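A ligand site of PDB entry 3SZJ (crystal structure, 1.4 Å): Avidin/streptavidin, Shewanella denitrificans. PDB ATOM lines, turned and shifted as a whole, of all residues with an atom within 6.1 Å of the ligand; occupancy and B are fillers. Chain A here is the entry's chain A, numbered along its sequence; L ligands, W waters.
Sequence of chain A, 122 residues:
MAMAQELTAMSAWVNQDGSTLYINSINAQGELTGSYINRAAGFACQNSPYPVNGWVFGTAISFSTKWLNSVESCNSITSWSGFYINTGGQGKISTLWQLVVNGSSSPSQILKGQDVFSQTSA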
ATOM      1  N   ASN A  15      37.654   3.695  21.221  1.00  0.00           N
ATOM      2  CA  ASN A  15      37.439   2.930  19.993  1.00  0.00           C
ATOM      3  C   ASN A  15      37.460   3.773  18.736  1.00  0.00           C
ATOM      4  O   ASN A  15      37.731   4.979  18.802  1.00  0.00           O
ATOM      5  CB  ASN A  15      36.196   2.016  20.055  1.00  0.00           C
ATOM      6  CG  ASN A  15      34.886   2.766  19.977  1.00  0.00           C
ATOM      7  OD1 ASN A  15      34.815   3.916  19.515  1.00  0.00           O
ATOM      8  ND2 ASN A  15      33.805   2.109  20.425  1.00  0.00           N
ATOM      9  N   GLN A  16      37.201   3.131  17.595  1.00  0.00           N
ATOM     10  CA  GLN A  16      37.362   3.793  16.307  1.00  0.00           C
ATOM     11  C   GLN A  16      36.339   4.891  16.079  1.00  0.00           C
ATOM     12  O   GLN A  16      36.481   5.712  15.146  1.00  0.00           O
ATOM     13  CB  GLN A  16      37.286   2.762  15.178  1.00  0.00           C
ATOM     14  CG  GLN A  16      35.874   2.182  14.957  1.00  0.00           C
ATOM     15  CD  GLN A  16      35.414   1.223  16.067  1.00  0.00           C
ATOM     16  OE1 GLN A  16      36.215   0.461  16.611  1.00  0.00           O
ATOM     17  NE2 GLN A  16      34.129   1.282  16.411  1.00  0.00           N
ATOM     18  N   ASP A  17      35.285   4.909  16.896  1.00  0.00           N
ATOM     19  CA  ASP A  17      34.248   5.950  16.816  1.00  0.00           C
ATOM     20  C   ASP A  17      34.452   7.050  17.857  1.00  0.00           C
ATOM     21  O   ASP A  17      33.685   8.009  17.920  1.00  0.00           O
ATOM     22  CB  ASP A  17      32.856   5.328  16.972  1.00  0.00           C
ATOM     23  CG  ASP A  17      32.402   4.673  15.703  1.00  0.00           C
ATOM     24  OD1 ASP A  17      31.938   5.409  14.792  1.00  0.00           O
ATOM     25  OD2 ASP A  17      32.520   3.441  15.582  1.00  0.00           O
ATOM     26  N   SER A  19      34.500   6.541  21.198  1.00  0.00           N
ATOM     27  CA  SER A  19      33.866   6.218  22.473  1.00  0.00           C
ATOM     28  C   SER A  19      34.918   5.751  23.462  1.00  0.00           C
ATOM     29  O   SER A  19      35.910   5.113  23.077  1.00  0.00           O
ATOM     30  CB  SER A  19      32.825   5.106  22.299  1.00  0.00           C
ATOM     31  OG  SER A  19      31.857   5.513  21.348  1.00  0.00           O
ATOM     32  N   THR A  20      34.704   6.049  24.746  1.00  0.00           N
ATOM     33  CA  THR A  20      35.685   5.707  25.764  1.00  0.00           C
ATOM     34  C   THR A  20      35.146   4.723  26.790  1.00  0.00           C
ATOM     35  O   THR A  20      34.052   4.922  27.310  1.00  0.00           O
ATOM     36  CB  THR A  20      36.141   6.967  26.490  1.00  0.00           C
ATOM     37  OG1 THR A  20      36.666   7.889  25.542  1.00  0.00           O
ATOM     38  CG2 THR A  20      37.238   6.634  27.507  1.00  0.00           C
ATOM     39  N   TYR A  36      31.256   4.235  30.650  1.00  0.00           N
ATOM     40  CA  TYR A  36      31.417   4.256  29.209  1.00  0.00           C
ATOM     41  C   TYR A  36      30.819   5.544  28.670  1.00  0.00           C
ATOM     42  O   TYR A  36      29.724   5.938  29.090  1.00  0.00           O
ATOM     43  CB  TYR A  36      30.645   3.076  28.608  1.00  0.00           C
ATOM     44  CG  TYR A  36      31.011   2.766  27.175  1.00  0.00           C
ATOM     45  CD1 TYR A  36      30.372   3.416  26.106  1.00  0.00           C
ATOM     46  CD2 TYR A  36      31.996   1.807  26.886  1.00  0.00           C
ATOM     47  CE1 TYR A  36      30.727   3.132  24.773  1.00  0.00           C
ATOM     48  CE2 TYR A  36      32.343   1.519  25.576  1.00  0.00           C
ATOM     49  CZ  TYR A  36      31.727   2.169  24.524  1.00  0.00           C
ATOM     50  OH  TYR A  36      32.089   1.842  23.240  1.00  0.00           O
ATOM     51  N   ILE A  37      31.527   6.179  27.724  1.00  0.00           N
ATOM     52  CA  ILE A  37      30.969   7.363  27.043  1.00  0.00           C
ATOM     53  C   ILE A  37      30.905   7.053  25.563  1.00  0.00           C
ATOM     54  O   ILE A  37      31.944   6.809  24.938  1.00  0.00           O
ATOM     55  CB  ILE A  37      31.820   8.644  27.290  1.00  0.00           C
ATOM     56  CG1 ILE A  37      31.893   8.986  28.783  1.00  0.00           C
ATOM     57  CG2 ILE A  37      31.272   9.823  26.463  1.00  0.00           C
ATOM     58  CD1 ILE A  37      32.823  10.178  29.074  1.00  0.00           C
ATOM     59  N   ASN A  38      29.690   7.038  25.019  1.00  0.00           N
ATOM     60  CA  ASN A  38      29.467   6.756  23.614  1.00  0.00           C
ATOM     61  C   ASN A  38      29.605   8.034  22.800  1.00  0.00           C
ATOM     62  O   ASN A  38      29.030   9.082  23.142  1.00  0.00           O
ATOM     63  CB  ASN A  38      28.037   6.195  23.465  1.00  0.00           C
ATOM     64  CG  ASN A  38      27.586   6.065  22.029  1.00  0.00           C
ATOM     65  OD1 ASN A  38      28.339   5.606  21.177  1.00  0.00           O
ATOM     66  ND2 ASN A  38      26.330   6.478  21.760  1.00  0.00           N
ATOM     67  N   ARG A  39      30.339   7.925  21.685  1.00  0.00           N
ATOM     68  CA  ARG A  39      30.494   9.043  20.733  1.00  0.00           C
ATOM     69  C   ARG A  39      30.250   8.599  19.291  1.00  0.00           C
ATOM     70  O   ARG A  39      30.666   9.304  18.354  1.00  0.00           O
ATOM     71  CB  ARG A  39      31.858   9.721  20.882  1.00  0.00           C
ATOM     72  CG  ARG A  39      32.051  10.296  22.266  1.00  0.00           C
ATOM     73  CD  ARG A  39      33.294  11.162  22.358  1.00  0.00           C
ATOM     74  NE  ARG A  39      33.533  11.631  23.724  1.00  0.00           N
ATOM     75  CZ  ARG A  39      34.219  10.958  24.643  1.00  0.00           C
ATOM     76  NH1 ARG A  39      34.725   9.757  24.354  1.00  0.00           N
ATOM     77  NH2 ARG A  39      34.386  11.468  25.858  1.00  0.00           N
ATOM     78  N   ALA A  40      29.603   7.450  19.106  1.00  0.00           N
ATOM     79  CA  ALA A  40      29.381   6.917  17.750  1.00  0.00           C
ATOM     80  C   ALA A  40      28.195   7.566  17.071  1.00  0.00           C
ATOM     81  O   ALA A  40      27.091   7.537  17.596  1.00  0.00           O
ATOM     82  CB  ALA A  40      29.208   5.401  17.780  1.00  0.00           C
ATOM     83  N   GLY A  42      25.097   7.853  14.715  1.00  0.00           N
ATOM     84  CA  GLY A  42      24.045   6.896  14.431  1.00  0.00           C
ATOM     85  C   GLY A  42      23.473   6.236  15.657  1.00  0.00           C
ATOM     86  O   GLY A  42      22.615   5.352  15.540  1.00  0.00           O
ATOM     87  N   PHE A  43      23.937   6.662  16.846  1.00  0.00           N
ATOM     88  CA  PHE A  43      23.427   6.166  18.111  1.00  0.00           C
ATOM     89  C   PHE A  43      23.121   7.342  19.001  1.00  0.00           C
ATOM     90  O   PHE A  43      23.839   8.358  18.941  1.00  0.00           O
ATOM     91  CB  PHE A  43      24.437   5.232  18.807  1.00  0.00           C
ATOM     92  CG  PHE A  43      24.708   3.958  18.046  1.00  0.00           C
ATOM     93  CD1 PHE A  43      25.729   3.917  17.105  1.00  0.00           C
ATOM     94  CD2 PHE A  43      23.959   2.806  18.263  1.00  0.00           C
ATOM     95  CE1 PHE A  43      26.009   2.754  16.382  1.00  0.00           C
ATOM     96  CE2 PHE A  43      24.224   1.625  17.537  1.00  0.00           C
ATOM     97  CZ  PHE A  43      25.262   1.604  16.609  1.00  0.00           C
ATOM     98  N   ALA A  44      22.069   7.233  19.812  1.00  0.00           N
ATOM     99  CA  ALA A  44      21.767   8.253  20.846  1.00  0.00           C
ATOM    100  C   ALA A  44      22.582   7.974  22.130  1.00  0.00           C
ATOM    101  O   ALA A  44      23.562   7.218  22.082  1.00  0.00           O
ATOM    102  CB  ALA A  44      20.243   8.350  21.111  1.00  0.00           C
ATOM    103  N   CYS A  45      22.233   8.602  23.239  1.00  0.00           N
ATOM    104  CA  CYS A  45      22.989   8.409  24.486  1.00  0.00           C
ATOM    105  C   CYS A  45      24.481   8.671  24.301  1.00  0.00           C
ATOM    106  O   CYS A  45      25.332   7.902  24.765  1.00  0.00           O
ATOM    107  CB  CYS A  45      22.762   7.004  25.083  1.00  0.00           C
ATOM    108  SG  CYS A  45      21.098   6.821  25.781  1.00  0.00           S
ATOM    109  N   THR A  65      27.151  -2.423  29.263  1.00  0.00           N
ATOM    110  CA  THR A  65      26.682  -1.094  29.687  1.00  0.00           C
ATOM    111  C   THR A  65      25.157  -1.051  29.580  1.00  0.00           C
ATOM    112  O   THR A  65      24.588  -1.498  28.570  1.00  0.00           O
ATOM    113  CB  THR A  65      27.255  -0.020  28.761  1.00  0.00           C
ATOM    114  OG1 THR A  65      26.855  -0.296  27.418  1.00  0.00           O
ATOM    115  CG2 THR A  65      28.776  -0.009  28.827  1.00  0.00           C
ATOM    116  N   TRP A  67      22.079   1.455  29.238  1.00  0.00           N
ATOM    117  CA  TRP A  67      21.978   2.827  28.717  1.00  0.00           C
ATOM    118  C   TRP A  67      20.883   3.629  29.449  1.00  0.00           C
ATOM    119  O   TRP A  67      19.893   4.091  28.854  1.00  0.00           O
ATOM    120  CB  TRP A  67      21.762   2.787  27.190  1.00  0.00           C
ATOM    121  CG  TRP A  67      22.907   2.121  26.453  1.00  0.00           C
ATOM    122  CD1 TRP A  67      22.903   0.857  25.864  1.00  0.00           C
ATOM    123  CD2 TRP A  67      24.220   2.668  26.222  1.00  0.00           C
ATOM    124  NE1 TRP A  67      24.137   0.597  25.331  1.00  0.00           N
ATOM    125  CE2 TRP A  67      24.957   1.690  25.506  1.00  0.00           C
ATOM    126  CE3 TRP A  67      24.838   3.884  26.534  1.00  0.00           C
ATOM    127  CZ2 TRP A  67      26.282   1.884  25.115  1.00  0.00           C
ATOM    128  CZ3 TRP A  67      26.163   4.071  26.155  1.00  0.00           C
ATOM    129  CH2 TRP A  67      26.866   3.080  25.448  1.00  0.00           C
ATOM    130  N   CYS A  74      18.269   5.237  26.706  1.00  0.00           N
ATOM    131  CA  CYS A  74      18.057   4.629  25.394  1.00  0.00           C
ATOM    132  C   CYS A  74      17.402   3.247  25.463  1.00  0.00           C
ATOM    133  O   CYS A  74      17.303   2.566  24.425  1.00  0.00           O
ATOM    134  CB  CYS A  74      19.382   4.555  24.611  1.00  0.00           C
ATOM    135  SG  CYS A  74      19.968   6.199  24.130  1.00  0.00           S
ATOM    136  N   ASN A  75      16.914   2.853  26.643  1.00  0.00           N
ATOM    137  CA  ASN A  75      16.037   1.658  26.746  1.00  0.00           C
ATOM    138  C   ASN A  75      16.736   0.375  26.262  1.00  0.00           C
ATOM    139  O   ASN A  75      16.094  -0.535  25.718  1.00  0.00           O
ATOM    140  CB  ASN A  75      14.771   1.918  25.898  1.00  0.00           C
ATOM    141  CG  ASN A  75      13.487   1.494  26.596  1.00  0.00           C
ATOM    142  OD1 ASN A  75      13.443   1.304  27.811  1.00  0.00           O
ATOM    143  ND2 ASN A  75      12.417   1.388  25.826  1.00  0.00           N
ATOM    144  N   SER A  76      18.045   0.260  26.504  1.00  0.00           N
ATOM    145  CA  SER A  76      18.829  -0.799  25.888  1.00  0.00           C
ATOM    146  C   SER A  76      20.050  -1.149  26.710  1.00  0.00           C
ATOM    147  O   SER A  76      20.404  -0.417  27.641  1.00  0.00           O
ATOM    148  CB  SER A  76      19.284  -0.368  24.480  1.00  0.00           C
ATOM    149  OG  SER A  76      18.182   0.067  23.713  1.00  0.00           O
ATOM    150  N   THR A  78      24.126  -2.840  25.957  1.00  0.00           N
ATOM    151  CA  THR A  78      25.156  -3.417  25.057  1.00  0.00           C
ATOM    152  C   THR A  78      26.099  -4.330  25.833  1.00  0.00           C
ATOM    153  O   THR A  78      26.446  -4.028  26.974  1.00  0.00           O
ATOM    154  CB  THR A  78      25.964  -2.306  24.352  1.00  0.00           C
ATOM    155  OG1 THR A  78      25.028  -1.493  23.646  1.00  0.00           O
ATOM    156  CG2 THR A  78      26.950  -2.913  23.331  1.00  0.00           C
ATOM    157  N   TRP A  80      29.794  -6.408  25.204  1.00  0.00           N
ATOM    158  CA  TRP A  80      30.985  -6.650  24.396  1.00  0.00           C
ATOM    159  C   TRP A  80      31.702  -7.895  24.905  1.00  0.00           C
ATOM    160  O   TRP A  80      31.828  -8.116  26.126  1.00  0.00           O
ATOM    161  CB  TRP A  80      31.970  -5.485  24.527  1.00  0.00           C
ATOM    162  CG  TRP A  80      31.609  -4.140  23.893  1.00  0.00           C
ATOM    163  CD1 TRP A  80      32.077  -3.642  22.696  1.00  0.00           C
ATOM    164  CD2 TRP A  80      30.759  -3.113  24.454  1.00  0.00           C
ATOM    165  NE1 TRP A  80      31.561  -2.360  22.475  1.00  0.00           N
ATOM    166  CE2 TRP A  80      30.770  -2.020  23.544  1.00  0.00           C
ATOM    167  CE3 TRP A  80      30.027  -3.004  25.662  1.00  0.00           C
ATOM    168  CZ2 TRP A  80      30.060  -0.837  23.812  1.00  0.00           C
ATOM    169  CZ3 TRP A  80      29.312  -1.834  25.912  1.00  0.00           C
ATOM    170  CH2 TRP A  80      29.338  -0.765  25.004  1.00  0.00           C
ATOM    171  N   TRP A  97      30.268  -6.873  19.632  1.00  0.00           N
ATOM    172  CA  TRP A  97      29.189  -6.430  20.546  1.00  0.00           C
ATOM    173  C   TRP A  97      27.780  -6.805  20.087  1.00  0.00           C
ATOM    174  O   TRP A  97      27.543  -7.038  18.882  1.00  0.00           O
ATOM    175  CB  TRP A  97      29.236  -4.938  20.844  1.00  0.00           C
ATOM    176  CG  TRP A  97      29.224  -4.001  19.648  1.00  0.00           C
ATOM    177  CD1 TRP A  97      30.307  -3.431  19.051  1.00  0.00           C
ATOM    178  CD2 TRP A  97      28.067  -3.523  18.934  1.00  0.00           C
ATOM    179  NE1 TRP A  97      29.903  -2.651  17.977  1.00  0.00           N
ATOM    180  CE2 TRP A  97      28.531  -2.684  17.899  1.00  0.00           C
ATOM    181  CE3 TRP A  97      26.686  -3.730  19.089  1.00  0.00           C
ATOM    182  CZ2 TRP A  97      27.648  -2.028  17.008  1.00  0.00           C
ATOM    183  CZ3 TRP A  97      25.819  -3.106  18.212  1.00  0.00           C
ATOM    184  CH2 TRP A  97      26.304  -2.261  17.171  1.00  0.00           C
ATOM    185  N   LEU A  99      23.614  -5.483  21.022  1.00  0.00           N
ATOM    186  CA  LEU A  99      22.783  -4.464  21.654  1.00  0.00           C
ATOM    187  C   LEU A  99      21.335  -4.958  21.640  1.00  0.00           C
ATOM    188  O   LEU A  99      20.797  -5.235  20.580  1.00  0.00           O
ATOM    189  CB  LEU A  99      22.937  -3.138  20.879  1.00  0.00           C
ATOM    190  CG  LEU A  99      22.108  -1.859  21.098  1.00  0.00           C
ATOM    191  CD1 LEU A  99      21.999  -1.420  22.542  1.00  0.00           C
ATOM    192  CD2 LEU A  99      22.709  -0.717  20.268  1.00  0.00           C
ATOM    193  N   VAL A 101      17.268  -4.327  23.014  1.00  0.00           N
ATOM    194  CA  VAL A 101      16.362  -3.243  23.367  1.00  0.00           C
ATOM    195  C   VAL A 101      15.177  -3.761  24.190  1.00  0.00           C
ATOM    196  O   VAL A 101      14.580  -4.793  23.879  1.00  0.00           O
ATOM    197  CB  VAL A 101      15.847  -2.518  22.096  1.00  0.00           C
ATOM    198  CG1 VAL A 101      15.014  -1.306  22.473  1.00  0.00           C
ATOM    199  CG2 VAL A 101      17.023  -2.088  21.199  1.00  0.00           C
ATOM    200  N   ASP A 115      33.999  -3.525  17.608  1.00  0.00           N
ATOM    201  CA  ASP A 115      34.743  -2.348  18.081  1.00  0.00           C
ATOM    202  C   ASP A 115      36.154  -2.778  18.449  1.00  0.00           C
ATOM    203  O   ASP A 115      36.357  -3.839  19.046  1.00  0.00           O
ATOM    204  CB  ASP A 115      34.171  -1.770  19.374  1.00  0.00           C
ATOM    205  CG  ASP A 115      32.899  -0.919  19.177  1.00  0.00           C
ATOM    206  OD1 ASP A 115      32.600  -0.466  18.044  1.00  0.00           O
ATOM    207  OD2 ASP A 115      32.219  -0.704  20.209  1.00  0.00           O
ATOM    208  N   PHE A 117      39.266  -1.123  20.637  1.00  0.00           N
ATOM    209  CA  PHE A 117      39.673  -0.059  21.555  1.00  0.00           C
ATOM    210  C   PHE A 117      41.189  -0.021  21.688  1.00  0.00           C
ATOM    211  O   PHE A 117      41.839  -1.080  21.769  1.00  0.00           O
ATOM    212  CB  PHE A 117      39.090  -0.321  22.953  1.00  0.00           C
ATOM    213  CG  PHE A 117      37.583  -0.303  23.025  1.00  0.00           C
ATOM    214  CD1 PHE A 117      36.842  -1.428  22.644  1.00  0.00           C
ATOM    215  CD2 PHE A 117      36.903   0.848  23.407  1.00  0.00           C
ATOM    216  CE1 PHE A 117      35.457  -1.423  22.717  1.00  0.00           C
ATOM    217  CE2 PHE A 117      35.506   0.846  23.483  1.00  0.00           C
ATOM    218  CZ  PHE A 117      34.796  -0.291  23.120  1.00  0.00           C
HETATM  219  C1  LIG L   1      21.591   3.124  22.011  1.00  0.00           C
HETATM  220  O1  LIG L   1      21.657   3.747  20.924  1.00  0.00           O
HETATM  221  O2  LIG L   1      20.743   2.223  22.144  1.00  0.00           O
HETATM  222  C2  LIG L   1      22.521   3.454  23.134  1.00  0.00           C
HETATM  223  C3  LIG L   1      23.954   3.728  22.636  1.00  0.00           C
HETATM  224  C4  LIG L   1      24.591   2.517  21.963  1.00  0.00           C
HETATM  225  C5  LIG L   1      26.022   2.781  21.467  1.00  0.00           C
HETATM  226  C6  LIG L   1      26.633   1.537  20.805  1.00  0.00           C
HETATM  227  S1  LIG L   1      27.203   0.392  21.890  1.00  0.00           S
HETATM  228  C7  LIG L   1      28.047  -0.462  20.540  1.00  0.00           C
HETATM  229  C8  LIG L   1      28.649   0.583  19.646  1.00  0.00           C
HETATM  230  N1  LIG L   1      29.955   1.016  20.092  1.00  0.00           N
HETATM  231  C9  LIG L   1      29.903   2.287  20.482  1.00  0.00           C
HETATM  232  O3  LIG L   1      30.964   2.961  21.080  1.00  0.00           O
HETATM  233  N2  LIG L   1      28.713   2.860  20.284  1.00  0.00           N
HETATM  234  C10 LIG L   1      27.780   1.833  19.847  1.00  0.00           C
HETATM  235  O   HOH W   1      19.977   5.259  19.046  1.00  0.00           O
HETATM  236  O   HOH W   2      18.731   1.580  20.429  1.00  0.00           O
HETATM  237  O   HOH W   3      30.188   1.404  16.734  1.00  0.00           O
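O3 of the ligand lies within hydrogen-bond range of OG of Ser 19 (2.7 Å). OH of Tyr 36 sits at hydrogen-bond distance from O3 of the ligand, at 2.7 Å. A nitrogen (N1) of the ligand sits at hydrogen-bond distance from the side-chain carboxylate (OD2) of Asp 115 (2.8 Å). The side-chain amide nitrogen of Asn 15 is in hydrogen-bond range of an oxygen (O3) of the ligand. OG1 of Thr 78 lies close to S1 of the ligand (3.4 Å). The side-chain amide oxygen (OD1) of Asn 38 lies within hydrogen-bond range of a nitrogen (N2) of the ligand (2.9 Å).
The side-chain carboxylate (OD2) of Asp 115 is in hydrogen-bond range of the indole nitrogen (NE1) of Trp 80 (2.9 Å). OG1 of Thr 78 sits at hydrogen-bond distance from NE1 of Trp 67 (2.8 Å). The backbone NH of Trp 67 sits at hydrogen-bond distance from the backbone carbonyl oxygen of Ser 76, at 3.0 Å. The backbone carbonyl oxygen (O) of Cys 74 lies within hydrogen-bond range of the side-chain hydroxyl (OG) of Ser 76, at 2.7 Å. The side-chain carboxylate of Asp 115 lies within hydrogen-bond range of the side-chain amide nitrogen of Asn 15 (3.2 Å). OD1 of Asn 15 lies within hydrogen-bond range of N of Asp 17. ND2 of Asn 38 lies within hydrogen-bond range of O of Ala 44, 2.9 Å away. The backbone NH of Ser 19 is in hydrogen-bond range of the side-chain amide oxygen of Asn 15, at 3.1 Å.
Ala 40 touches the ligand (CB to N2, 3.6 Å). CD2 of Phe 43 touches O1 of the ligand (3.6 Å). Ala 44 touches the ligand. Trp 67 touches the ligand (CG to C2, 3.6 Å). CB of Cys 74 touches C2 of the ligand, at 3.6 Å. OG of Ser 76 touches O2 of the ligand, 3.7 Å away. Trp 80 touches the ligand. Trp 97 touches the ligand (CD2 to C7, 3.5 Å). Leu 99 touches the ligand (CD1 to O2, 3.9 Å). Hydrophobic or aromatic side chains that line the ligand: Tyr 36, Ala 40, Phe 43, Trp 67, Trp 80, Trp 97 and Leu 99. Of the 26 residues printed, 15 come within 4 Å of the ligand.
Water W1 bridges an oxygen (O1) of the ligand and the backbone NH (N) of Ala 44. Water W3 lies within hydrogen-bond range of the side-chain carboxylate of Asp 17 (3.3 Å), the side-chain carboxylate of Asp 115 (3.3 Å) and a nitrogen (N1) of the ligand (3.4 Å).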
